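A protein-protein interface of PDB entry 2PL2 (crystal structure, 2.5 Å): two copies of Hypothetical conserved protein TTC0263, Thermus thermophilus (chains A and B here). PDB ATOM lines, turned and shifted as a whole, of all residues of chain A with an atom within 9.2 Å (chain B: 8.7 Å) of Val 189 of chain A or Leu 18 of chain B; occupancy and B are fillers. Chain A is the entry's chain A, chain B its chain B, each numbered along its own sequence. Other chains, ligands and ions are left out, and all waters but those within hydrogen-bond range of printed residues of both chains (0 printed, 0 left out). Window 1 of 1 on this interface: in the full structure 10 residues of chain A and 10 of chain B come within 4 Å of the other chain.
No position is printed for both chains.
Of the 7 pairs that touch across the chains among the printed residues, none has its exchanged pair printed and touching as well.
Hydrophobic or aromatic side chains of chain B that line the printed part of chain A: Leu 15 and Leu 18.
Of the 20 printed residues of chain A, 5 touch a printed residue of chain B.
Among the printed residues, 7 pairs touch across the chains.
Among the printed residues, Asp or Glu carboxylates within 4 Å of a Lys or Arg side-chain nitrogen of the other chain: Glu 159 of chain A with Arg 20 of chain B (2.5 Å).
NH2 of Arg 20 of chain B touches CD1 of Leu 162 of chain A, 3.6 Å away.
Val 189 of chain A touches Leu 18 of chain B.
Ser 193 of chain A touches Leu 15 of chain B.
CD1 of Leu 18 of chain B touches OG of Ser 193 of chain A, 3.96 Å away.
OG of Ser 193 of chain A touches CG of Arg 20 of chain B, at 3.3 Å.
The side-chain carboxylate (OE2) of Glu 159 of chain A lies within hydrogen-bond range of the side-chain hydroxyl (OH) of Tyr 174 of chain A, 3.2 Å away.
The side-chain carboxylate of Asp 186 of chain A lies within salt-bridge range of the guanidinium group of Arg 190 of chain A (3.4 Å).
N of Arg 20 of chain B is in hydrogen-bond range of O of Leu 15 of chain B, 3.0 Å away.
Of chain B, only Leu 18 (3.2 Å) comes within 4 Å of Val 189 of chain A.
No residue of chain A comes within 4 Å of Gly 19 of chain B.
Of the printed residues of chain B, Leu 162 of chain A touches Arg 20.
Of the printed residues of chain A, Leu 15 of chain B touches Ser 193 (3.2 Å).
Of the printed residues of chain B, Arg 190 of chain A touches Arg 20 (3.3 Å).
Of the printed residues of chain A, Arg 20 of chain B touches Glu 159 (2.5 Å), Leu 162 (3.6 Å), Arg 190 (3.3 Å) and Ser 193 (3.3 Å).
Leu 185 of chain A touches none of the printed residues of chain B.
Tyr 16 of chain B touches none of the printed residues of chain A.
The nearest printed residue of chain B that does not touch Ser 193 of chain A is Gln 14 of chain B (6.7 Å).
The side-chain carboxylate (OE2) of Glu 159 of chain A lies within salt-bridge range of the guanidinium group (NH2) of Arg 20 of chain B (2.5 Å).
NH1 of Arg 20 of chain B sits close to NH1 of Arg 190 of chain A.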
ATOM      1  N   GLU A 159       2.609   0.922 -24.303  1.00  0.00           N
ATOM      2  CA  GLU A 159       3.026   2.097 -25.066  1.00  0.00           C
ATOM      3  C   GLU A 159       1.915   2.651 -25.924  1.00  0.00           C
ATOM      4  O   GLU A 159       1.710   3.860 -25.949  1.00  0.00           O
ATOM      5  CB  GLU A 159       4.232   1.760 -25.942  1.00  0.00           C
ATOM      6  CG  GLU A 159       5.549   1.939 -25.227  1.00  0.00           C
ATOM      7  CD  GLU A 159       5.770   3.379 -24.812  1.00  0.00           C
ATOM      8  OE1 GLU A 159       5.869   4.237 -25.710  1.00  0.00           O
ATOM      9  OE2 GLU A 159       5.844   3.650 -23.596  1.00  0.00           O
ATOM     10  N   LEU A 162      -0.509   4.600 -23.783  1.00  0.00           N
ATOM     11  CA  LEU A 162      -0.076   5.915 -23.335  1.00  0.00           C
ATOM     12  C   LEU A 162      -0.322   6.903 -24.471  1.00  0.00           C
ATOM     13  O   LEU A 162      -0.707   8.049 -24.242  1.00  0.00           O
ATOM     14  CB  LEU A 162       1.402   5.895 -22.935  1.00  0.00           C
ATOM     15  CG  LEU A 162       1.637   5.274 -21.554  1.00  0.00           C
ATOM     16  CD1 LEU A 162       3.104   5.293 -21.201  1.00  0.00           C
ATOM     17  CD2 LEU A 162       0.842   6.052 -20.525  1.00  0.00           C
ATOM     18  N   LEU A 171      -0.874   1.031 -17.547  1.00  0.00           N
ATOM     19  CA  LEU A 171      -0.328   0.564 -16.282  1.00  0.00           C
ATOM     20  C   LEU A 171      -0.668  -0.912 -16.070  1.00  0.00           C
ATOM     21  O   LEU A 171       0.170  -1.686 -15.613  1.00  0.00           O
ATOM     22  CB  LEU A 171      -0.886   1.417 -15.134  1.00  0.00           C
ATOM     23  CG  LEU A 171      -0.550   2.912 -15.223  1.00  0.00           C
ATOM     24  CD1 LEU A 171      -1.354   3.681 -14.212  1.00  0.00           C
ATOM     25  CD2 LEU A 171       0.933   3.124 -14.998  1.00  0.00           C
ATOM     26  N   TYR A 174       1.673  -3.126 -18.006  1.00  0.00           N
ATOM     27  CA  TYR A 174       3.032  -3.189 -17.459  1.00  0.00           C
ATOM     28  C   TYR A 174       3.029  -4.143 -16.266  1.00  0.00           C
ATOM     29  O   TYR A 174       3.929  -4.984 -16.115  1.00  0.00           O
ATOM     30  CB  TYR A 174       3.522  -1.795 -17.017  1.00  0.00           C
ATOM     31  CG  TYR A 174       3.977  -0.889 -18.152  1.00  0.00           C
ATOM     32  CD1 TYR A 174       4.963  -1.299 -19.040  1.00  0.00           C
ATOM     33  CD2 TYR A 174       3.471   0.396 -18.293  1.00  0.00           C
ATOM     34  CE1 TYR A 174       5.431  -0.462 -20.032  1.00  0.00           C
ATOM     35  CE2 TYR A 174       3.931   1.250 -19.282  1.00  0.00           C
ATOM     36  CZ  TYR A 174       4.920   0.814 -20.153  1.00  0.00           C
ATOM     37  OH  TYR A 174       5.399   1.640 -21.151  1.00  0.00           O
ATOM     38  N   LEU A 178       5.315  -7.270 -16.038  1.00  0.00           N
ATOM     39  CA  LEU A 178       6.227  -7.454 -14.902  1.00  0.00           C
ATOM     40  C   LEU A 178       6.006  -8.750 -14.128  1.00  0.00           C
ATOM     41  O   LEU A 178       6.884  -9.180 -13.390  1.00  0.00           O
ATOM     42  CB  LEU A 178       6.167  -6.250 -13.955  1.00  0.00           C
ATOM     43  CG  LEU A 178       7.155  -5.159 -14.397  1.00  0.00           C
ATOM     44  CD1 LEU A 178       6.816  -3.846 -13.756  1.00  0.00           C
ATOM     45  CD2 LEU A 178       8.584  -5.602 -14.052  1.00  0.00           C
ATOM     46  N   PRO A 182       9.502 -10.369 -13.515  1.00  0.00           N
ATOM     47  CA  PRO A 182       9.588  -9.490 -12.333  1.00  0.00           C
ATOM     48  C   PRO A 182      10.938  -8.790 -12.078  1.00  0.00           C
ATOM     49  O   PRO A 182      10.987  -7.728 -11.444  1.00  0.00           O
ATOM     50  CB  PRO A 182       9.187 -10.422 -11.192  1.00  0.00           C
ATOM     51  CG  PRO A 182       9.778 -11.722 -11.629  1.00  0.00           C
ATOM     52  CD  PRO A 182       9.388 -11.782 -13.108  1.00  0.00           C
ATOM     53  N   LYS A 183      12.029  -9.382 -12.543  1.00  0.00           N
ATOM     54  CA  LYS A 183      13.336  -8.760 -12.349  1.00  0.00           C
ATOM     55  C   LYS A 183      13.767  -7.935 -13.561  1.00  0.00           C
ATOM     56  O   LYS A 183      14.955  -7.684 -13.748  1.00  0.00           O
ATOM     57  CB  LYS A 183      14.395  -9.823 -12.049  1.00  0.00           C
ATOM     58  CG  LYS A 183      14.130 -10.554 -10.750  1.00  0.00           C
ATOM     59  CD  LYS A 183      15.281 -11.427 -10.302  1.00  0.00           C
ATOM     60  CE  LYS A 183      14.898 -12.174  -9.020  1.00  0.00           C
ATOM     61  NZ  LYS A 183      16.018 -12.984  -8.468  1.00  0.00           N
ATOM     62  N   ASP A 184      12.802  -7.509 -14.375  1.00  0.00           N
ATOM     63  CA  ASP A 184      13.099  -6.730 -15.575  1.00  0.00           C
ATOM     64  C   ASP A 184      13.149  -5.235 -15.279  1.00  0.00           C
ATOM     65  O   ASP A 184      12.110  -4.551 -15.176  1.00  0.00           O
ATOM     66  CB  ASP A 184      12.059  -7.000 -16.673  1.00  0.00           C
ATOM     67  CG  ASP A 184      12.447  -6.384 -18.014  1.00  0.00           C
ATOM     68  OD1 ASP A 184      13.136  -5.341 -18.023  1.00  0.00           O
ATOM     69  OD2 ASP A 184      12.044  -6.932 -19.063  1.00  0.00           O
ATOM     70  N   LEU A 185      14.371  -4.724 -15.172  1.00  0.00           N
ATOM     71  CA  LEU A 185      14.568  -3.314 -14.871  1.00  0.00           C
ATOM     72  C   LEU A 185      14.059  -2.422 -15.987  1.00  0.00           C
ATOM     73  O   LEU A 185      13.472  -1.371 -15.736  1.00  0.00           O
ATOM     74  CB  LEU A 185      16.041  -3.058 -14.571  1.00  0.00           C
ATOM     75  CG  LEU A 185      16.558  -3.963 -13.435  1.00  0.00           C
ATOM     76  CD1 LEU A 185      17.909  -3.455 -12.926  1.00  0.00           C
ATOM     77  CD2 LEU A 185      15.548  -3.996 -12.296  1.00  0.00           C
ATOM     78  N   ASP A 186      14.262  -2.854 -17.224  1.00  0.00           N
ATOM     79  CA  ASP A 186      13.791  -2.096 -18.360  1.00  0.00           C
ATOM     80  C   ASP A 186      12.308  -1.871 -18.124  1.00  0.00           C
ATOM     81  O   ASP A 186      11.801  -0.755 -18.186  1.00  0.00           O
ATOM     82  CB  ASP A 186      14.006  -2.901 -19.636  1.00  0.00           C
ATOM     83  CG  ASP A 186      13.415  -2.216 -20.857  1.00  0.00           C
ATOM     84  OD1 ASP A 186      13.941  -1.153 -21.263  1.00  0.00           O
ATOM     85  OD2 ASP A 186      12.408  -2.732 -21.399  1.00  0.00           O
ATOM     86  N   LEU A 187      11.616  -2.959 -17.832  1.00  0.00           N
ATOM     87  CA  LEU A 187      10.185  -2.911 -17.561  1.00  0.00           C
ATOM     88  C   LEU A 187       9.829  -2.035 -16.337  1.00  0.00           C
ATOM     89  O   LEU A 187       8.886  -1.239 -16.393  1.00  0.00           O
ATOM     90  CB  LEU A 187       9.669  -4.343 -17.375  1.00  0.00           C
ATOM     91  CG  LEU A 187       8.282  -4.659 -17.940  1.00  0.00           C
ATOM     92  CD1 LEU A 187       8.103  -4.030 -19.307  1.00  0.00           C
ATOM     93  CD2 LEU A 187       8.125  -6.174 -18.004  1.00  0.00           C
ATOM     94  N   ARG A 188      10.589  -2.157 -15.249  1.00  0.00           N
ATOM     95  CA  ARG A 188      10.311  -1.362 -14.045  1.00  0.00           C
ATOM     96  C   ARG A 188      10.371   0.130 -14.300  1.00  0.00           C
ATOM     97  O   ARG A 188       9.511   0.877 -13.847  1.00  0.00           O
ATOM     98  CB  ARG A 188      11.276  -1.727 -12.925  1.00  0.00           C
ATOM     99  CG  ARG A 188      11.113  -3.143 -12.442  1.00  0.00           C
ATOM    100  CD  ARG A 188      12.087  -3.449 -11.323  1.00  0.00           C
ATOM    101  NE  ARG A 188      11.843  -4.765 -10.742  1.00  0.00           N
ATOM    102  CZ  ARG A 188      12.654  -5.350  -9.873  1.00  0.00           C
ATOM    103  NH1 ARG A 188      13.754  -4.728  -9.487  1.00  0.00           N
ATOM    104  NH2 ARG A 188      12.376  -6.558  -9.410  1.00  0.00           N
ATOM    105  N   VAL A 189      11.380   0.567 -15.044  1.00  0.00           N
ATOM    106  CA  VAL A 189      11.520   1.979 -15.373  1.00  0.00           C
ATOM    107  C   VAL A 189      10.335   2.513 -16.183  1.00  0.00           C
ATOM    108  O   VAL A 189       9.879   3.624 -15.947  1.00  0.00           O
ATOM    109  CB  VAL A 189      12.828   2.250 -16.180  1.00  0.00           C
ATOM    110  CG1 VAL A 189      12.926   3.760 -16.540  1.00  0.00           C
ATOM    111  CG2 VAL A 189      14.046   1.830 -15.364  1.00  0.00           C
ATOM    112  N   ARG A 190       9.836   1.741 -17.145  1.00  0.00           N
ATOM    113  CA  ARG A 190       8.714   2.216 -17.950  1.00  0.00           C
ATOM    114  C   ARG A 190       7.482   2.307 -17.080  1.00  0.00           C
ATOM    115  O   ARG A 190       6.709   3.253 -17.184  1.00  0.00           O
ATOM    116  CB  ARG A 190       8.447   1.272 -19.126  1.00  0.00           C
ATOM    117  CG  ARG A 190       9.482   1.352 -20.243  1.00  0.00           C
ATOM    118  CD  ARG A 190       9.534   0.040 -20.993  1.00  0.00           C
ATOM    119  NE  ARG A 190      10.567   0.020 -22.022  1.00  0.00           N
ATOM    120  CZ  ARG A 190      10.418   0.522 -23.246  1.00  0.00           C
ATOM    121  NH1 ARG A 190       9.266   1.089 -23.603  1.00  0.00           N
ATOM    122  NH2 ARG A 190      11.425   0.456 -24.116  1.00  0.00           N
ATOM    123  N   TYR A 191       7.303   1.310 -16.218  1.00  0.00           N
ATOM    124  CA  TYR A 191       6.158   1.273 -15.310  1.00  0.00           C
ATOM    125  C   TYR A 191       6.230   2.493 -14.403  1.00  0.00           C
ATOM    126  O   TYR A 191       5.259   3.246 -14.272  1.00  0.00           O
ATOM    127  CB  TYR A 191       6.215  -0.009 -14.488  1.00  0.00           C
ATOM    128  CG  TYR A 191       5.019  -0.249 -13.620  1.00  0.00           C
ATOM    129  CD1 TYR A 191       3.740   0.116 -14.039  1.00  0.00           C
ATOM    130  CD2 TYR A 191       5.151  -0.924 -12.406  1.00  0.00           C
ATOM    131  CE1 TYR A 191       2.626  -0.195 -13.273  1.00  0.00           C
ATOM    132  CE2 TYR A 191       4.051  -1.237 -11.641  1.00  0.00           C
ATOM    133  CZ  TYR A 191       2.791  -0.875 -12.078  1.00  0.00           C
ATOM    134  OH  TYR A 191       1.698  -1.218 -11.328  1.00  0.00           O
ATOM    135  N   ALA A 192       7.403   2.697 -13.804  1.00  0.00           N
ATOM    136  CA  ALA A 192       7.633   3.843 -12.914  1.00  0.00           C
ATOM    137  C   ALA A 192       7.355   5.143 -13.651  1.00  0.00           C
ATOM    138  O   ALA A 192       6.521   5.951 -13.237  1.00  0.00           O
ATOM    139  CB  ALA A 192       9.078   3.838 -12.395  1.00  0.00           C
ATOM    140  N   SER A 193       8.049   5.339 -14.762  1.00  0.00           N
ATOM    141  CA  SER A 193       7.861   6.552 -15.536  1.00  0.00           C
ATOM    142  C   SER A 193       6.398   6.746 -15.923  1.00  0.00           C
ATOM    143  O   SER A 193       5.908   7.877 -15.988  1.00  0.00           O
ATOM    144  CB  SER A 193       8.737   6.515 -16.785  1.00  0.00           C
ATOM    145  OG  SER A 193       8.700   7.767 -17.428  1.00  0.00           O
ATOM    146  N   ALA A 194       5.697   5.644 -16.170  1.00  0.00           N
ATOM    147  CA  ALA A 194       4.289   5.727 -16.530  1.00  0.00           C
ATOM    148  C   ALA A 194       3.490   6.134 -15.299  1.00  0.00           C
ATOM    149  O   ALA A 194       2.600   6.970 -15.399  1.00  0.00           O
ATOM    150  CB  ALA A 194       3.791   4.389 -17.079  1.00  0.00           C
ATOM    151  N   LEU A 195       3.804   5.544 -14.144  1.00  0.00           N
ATOM    152  CA  LEU A 195       3.103   5.877 -12.900  1.00  0.00           C
ATOM    153  C   LEU A 195       3.218   7.380 -12.667  1.00  0.00           C
ATOM    154  O   LEU A 195       2.315   7.998 -12.107  1.00  0.00           O
ATOM    155  CB  LEU A 195       3.681   5.082 -11.712  1.00  0.00           C
ATOM    156  CG  LEU A 195       3.287   3.595 -11.636  1.00  0.00           C
ATOM    157  CD1 LEU A 195       4.132   2.876 -10.596  1.00  0.00           C
ATOM    158  CD2 LEU A 195       1.804   3.470 -11.305  1.00  0.00           C
ATOM    159  N   LEU A 196       4.311   7.976 -13.132  1.00  0.00           N
ATOM    160  CA  LEU A 196       4.488   9.415 -12.998  1.00  0.00           C
ATOM    161  C   LEU A 196       3.414  10.090 -13.816  1.00  0.00           C
ATOM    162  O   LEU A 196       3.444  11.305 -14.015  1.00  0.00           O
ATOM    163  CB  LEU A 196       5.858   9.847 -13.511  1.00  0.00           C
ATOM    164  CG  LEU A 196       7.063   9.629 -12.586  1.00  0.00           C
ATOM    165  CD1 LEU A 196       8.351  10.091 -13.293  1.00  0.00           C
ATOM    166  CD2 LEU A 196       6.851  10.413 -11.282  1.00  0.00           C
ATOM    167  N   LEU B  11      10.774  18.515 -16.291  1.00  0.00           N
ATOM    168  CA  LEU B  11      10.198  17.185 -16.426  1.00  0.00           C
ATOM    169  C   LEU B  11      10.889  16.376 -17.508  1.00  0.00           C
ATOM    170  O   LEU B  11      11.089  15.166 -17.360  1.00  0.00           O
ATOM    171  CB  LEU B  11       8.703  17.287 -16.735  1.00  0.00           C
ATOM    172  CG  LEU B  11       7.960  15.953 -16.859  1.00  0.00           C
ATOM    173  CD1 LEU B  11       8.274  15.058 -15.660  1.00  0.00           C
ATOM    174  CD2 LEU B  11       6.462  16.214 -16.977  1.00  0.00           C
ATOM    175  N   GLY B  12      11.248  17.040 -18.601  1.00  0.00           N
ATOM    176  CA  GLY B  12      11.929  16.353 -19.686  1.00  0.00           C
ATOM    177  C   GLY B  12      13.286  15.851 -19.238  1.00  0.00           C
ATOM    178  O   GLY B  12      13.690  14.729 -19.551  1.00  0.00           O
ATOM    179  N   VAL B  13      14.002  16.679 -18.491  1.00  0.00           N
ATOM    180  CA  VAL B  13      15.320  16.279 -18.020  1.00  0.00           C
ATOM    181  C   VAL B  13      15.219  14.989 -17.234  1.00  0.00           C
ATOM    182  O   VAL B  13      16.045  14.087 -17.387  1.00  0.00           O
ATOM    183  CB  VAL B  13      15.952  17.355 -17.133  1.00  0.00           C
ATOM    184  CG1 VAL B  13      17.321  16.874 -16.638  1.00  0.00           C
ATOM    185  CG2 VAL B  13      16.101  18.654 -17.933  1.00  0.00           C
ATOM    186  N   GLN B  14      14.189  14.908 -16.400  1.00  0.00           N
ATOM    187  CA  GLN B  14      13.962  13.724 -15.587  1.00  0.00           C
ATOM    188  C   GLN B  14      13.590  12.564 -16.507  1.00  0.00           C
ATOM    189  O   GLN B  14      14.149  11.474 -16.380  1.00  0.00           O
ATOM    190  CB  GLN B  14      12.867  14.012 -14.546  1.00  0.00           C
ATOM    191  CG  GLN B  14      13.131  15.306 -13.786  1.00  0.00           C
ATOM    192  CD  GLN B  14      12.141  15.592 -12.668  1.00  0.00           C
ATOM    193  OE1 GLN B  14      10.936  15.509 -12.862  1.00  0.00           O
ATOM    194  NE2 GLN B  14      12.656  15.953 -11.497  1.00  0.00           N
ATOM    195  N   LEU B  15      12.670  12.781 -17.445  1.00  0.00           N
ATOM    196  CA  LEU B  15      12.325  11.695 -18.361  1.00  0.00           C
ATOM    197  C   LEU B  15      13.551  11.290 -19.193  1.00  0.00           C
ATOM    198  O   LEU B  15      13.780  10.096 -19.418  1.00  0.00           O
ATOM    199  CB  LEU B  15      11.171  12.089 -19.285  1.00  0.00           C
ATOM    200  CG  LEU B  15       9.799  12.130 -18.602  1.00  0.00           C
ATOM    201  CD1 LEU B  15       8.713  12.362 -19.643  1.00  0.00           C
ATOM    202  CD2 LEU B  15       9.558  10.825 -17.865  1.00  0.00           C
ATOM    203  N   TYR B  16      14.343  12.266 -19.642  1.00  0.00           N
ATOM    204  CA  TYR B  16      15.515  11.917 -20.418  1.00  0.00           C
ATOM    205  C   TYR B  16      16.355  10.977 -19.571  1.00  0.00           C
ATOM    206  O   TYR B  16      16.764   9.917 -20.041  1.00  0.00           O
ATOM    207  CB  TYR B  16      16.346  13.159 -20.797  1.00  0.00           C
ATOM    208  CG  TYR B  16      17.607  12.844 -21.607  1.00  0.00           C
ATOM    209  CD1 TYR B  16      17.662  13.064 -22.994  1.00  0.00           C
ATOM    210  CD2 TYR B  16      18.742  12.312 -20.984  1.00  0.00           C
ATOM    211  CE1 TYR B  16      18.830  12.766 -23.736  1.00  0.00           C
ATOM    212  CE2 TYR B  16      19.900  12.007 -21.709  1.00  0.00           C
ATOM    213  CZ  TYR B  16      19.939  12.236 -23.081  1.00  0.00           C
ATOM    214  OH  TYR B  16      21.103  11.942 -23.763  1.00  0.00           O
ATOM    215  N   ALA B  17      16.602  11.364 -18.322  1.00  0.00           N
ATOM    216  CA  ALA B  17      17.397  10.552 -17.405  1.00  0.00           C
ATOM    217  C   ALA B  17      16.817   9.154 -17.200  1.00  0.00           C
ATOM    218  O   ALA B  17      17.562   8.206 -16.943  1.00  0.00           O
ATOM    219  CB  ALA B  17      17.536  11.258 -16.054  1.00  0.00           C
ATOM    220  N   LEU B  18      15.495   9.025 -17.296  1.00  0.00           N
ATOM    221  CA  LEU B  18      14.843   7.724 -17.128  1.00  0.00           C
ATOM    222  C   LEU B  18      14.899   6.906 -18.419  1.00  0.00           C
ATOM    223  O   LEU B  18      14.652   5.694 -18.416  1.00  0.00           O
ATOM    224  CB  LEU B  18      13.392   7.913 -16.688  1.00  0.00           C
ATOM    225  CG  LEU B  18      13.193   8.617 -15.339  1.00  0.00           C
ATOM    226  CD1 LEU B  18      11.706   8.710 -15.030  1.00  0.00           C
ATOM    227  CD2 LEU B  18      13.904   7.845 -14.242  1.00  0.00           C
ATOM    228  N   GLY B  19      15.232   7.576 -19.523  1.00  0.00           N
ATOM    229  CA  GLY B  19      15.345   6.899 -20.809  1.00  0.00           C
ATOM    230  C   GLY B  19      14.106   6.952 -21.682  1.00  0.00           C
ATOM    231  O   GLY B  19      14.001   6.189 -22.636  1.00  0.00           O
ATOM    232  N   ARG B  20      13.177   7.845 -21.343  1.00  0.00           N
ATOM    233  CA  ARG B  20      11.919   8.026 -22.067  1.00  0.00           C
ATOM    234  C   ARG B  20      12.090   9.222 -22.997  1.00  0.00           C
ATOM    235  O   ARG B  20      11.524  10.297 -22.779  1.00  0.00           O
ATOM    236  CB  ARG B  20      10.778   8.283 -21.068  1.00  0.00           C
ATOM    237  CG  ARG B  20      10.572   7.147 -20.063  1.00  0.00           C
ATOM    238  CD  ARG B  20      10.040   5.886 -20.732  1.00  0.00           C
ATOM    239  NE  ARG B  20       8.615   6.006 -21.041  1.00  0.00           N
ATOM    240  CZ  ARG B  20       7.937   5.165 -21.822  1.00  0.00           C
ATOM    241  NH1 ARG B  20       8.544   4.129 -22.395  1.00  0.00           N
ATOM    242  NH2 ARG B  20       6.640   5.356 -22.017  1.00  0.00           N
ATOM    243  N   TYR B  21      12.879   9.008 -24.045  1.00  0.00           N
ATOM    244  CA  TYR B  21      13.219  10.043 -25.014  1.00  0.00           C
ATOM    245  C   TYR B  21      12.092  10.641 -25.844  1.00  0.00           C
ATOM    246  O   TYR B  21      12.058  11.850 -26.043  1.00  0.00           O
ATOM    247  CB  TYR B  21      14.336   9.508 -25.899  1.00  0.00           C
ATOM    248  CG  TYR B  21      15.508   8.992 -25.083  1.00  0.00           C
ATOM    249  CD1 TYR B  21      16.221   9.842 -24.228  1.00  0.00           C
ATOM    250  CD2 TYR B  21      15.895   7.663 -25.156  1.00  0.00           C
ATOM    251  CE1 TYR B  21      17.302   9.376 -23.466  1.00  0.00           C
ATOM    252  CE2 TYR B  21      16.963   7.187 -24.411  1.00  0.00           C
ATOM    253  CZ  TYR B  21      17.663   8.047 -23.560  1.00  0.00           C
ATOM    254  OH  TYR B  21      18.712   7.557 -22.806  1.00  0.00           O
ATOM    255  N   ALA B  24      10.302  12.880 -23.570  1.00  0.00           N
ATOM    256  CA  ALA B  24      11.141  14.012 -23.212  1.00  0.00           C
ATOM    257  C   ALA B  24      11.161  14.975 -24.398  1.00  0.00           C
ATOM    258  O   ALA B  24      11.125  16.197 -24.221  1.00  0.00           O
ATOM    259  CB  ALA B  24      12.551  13.538 -22.882  1.00  0.00           C
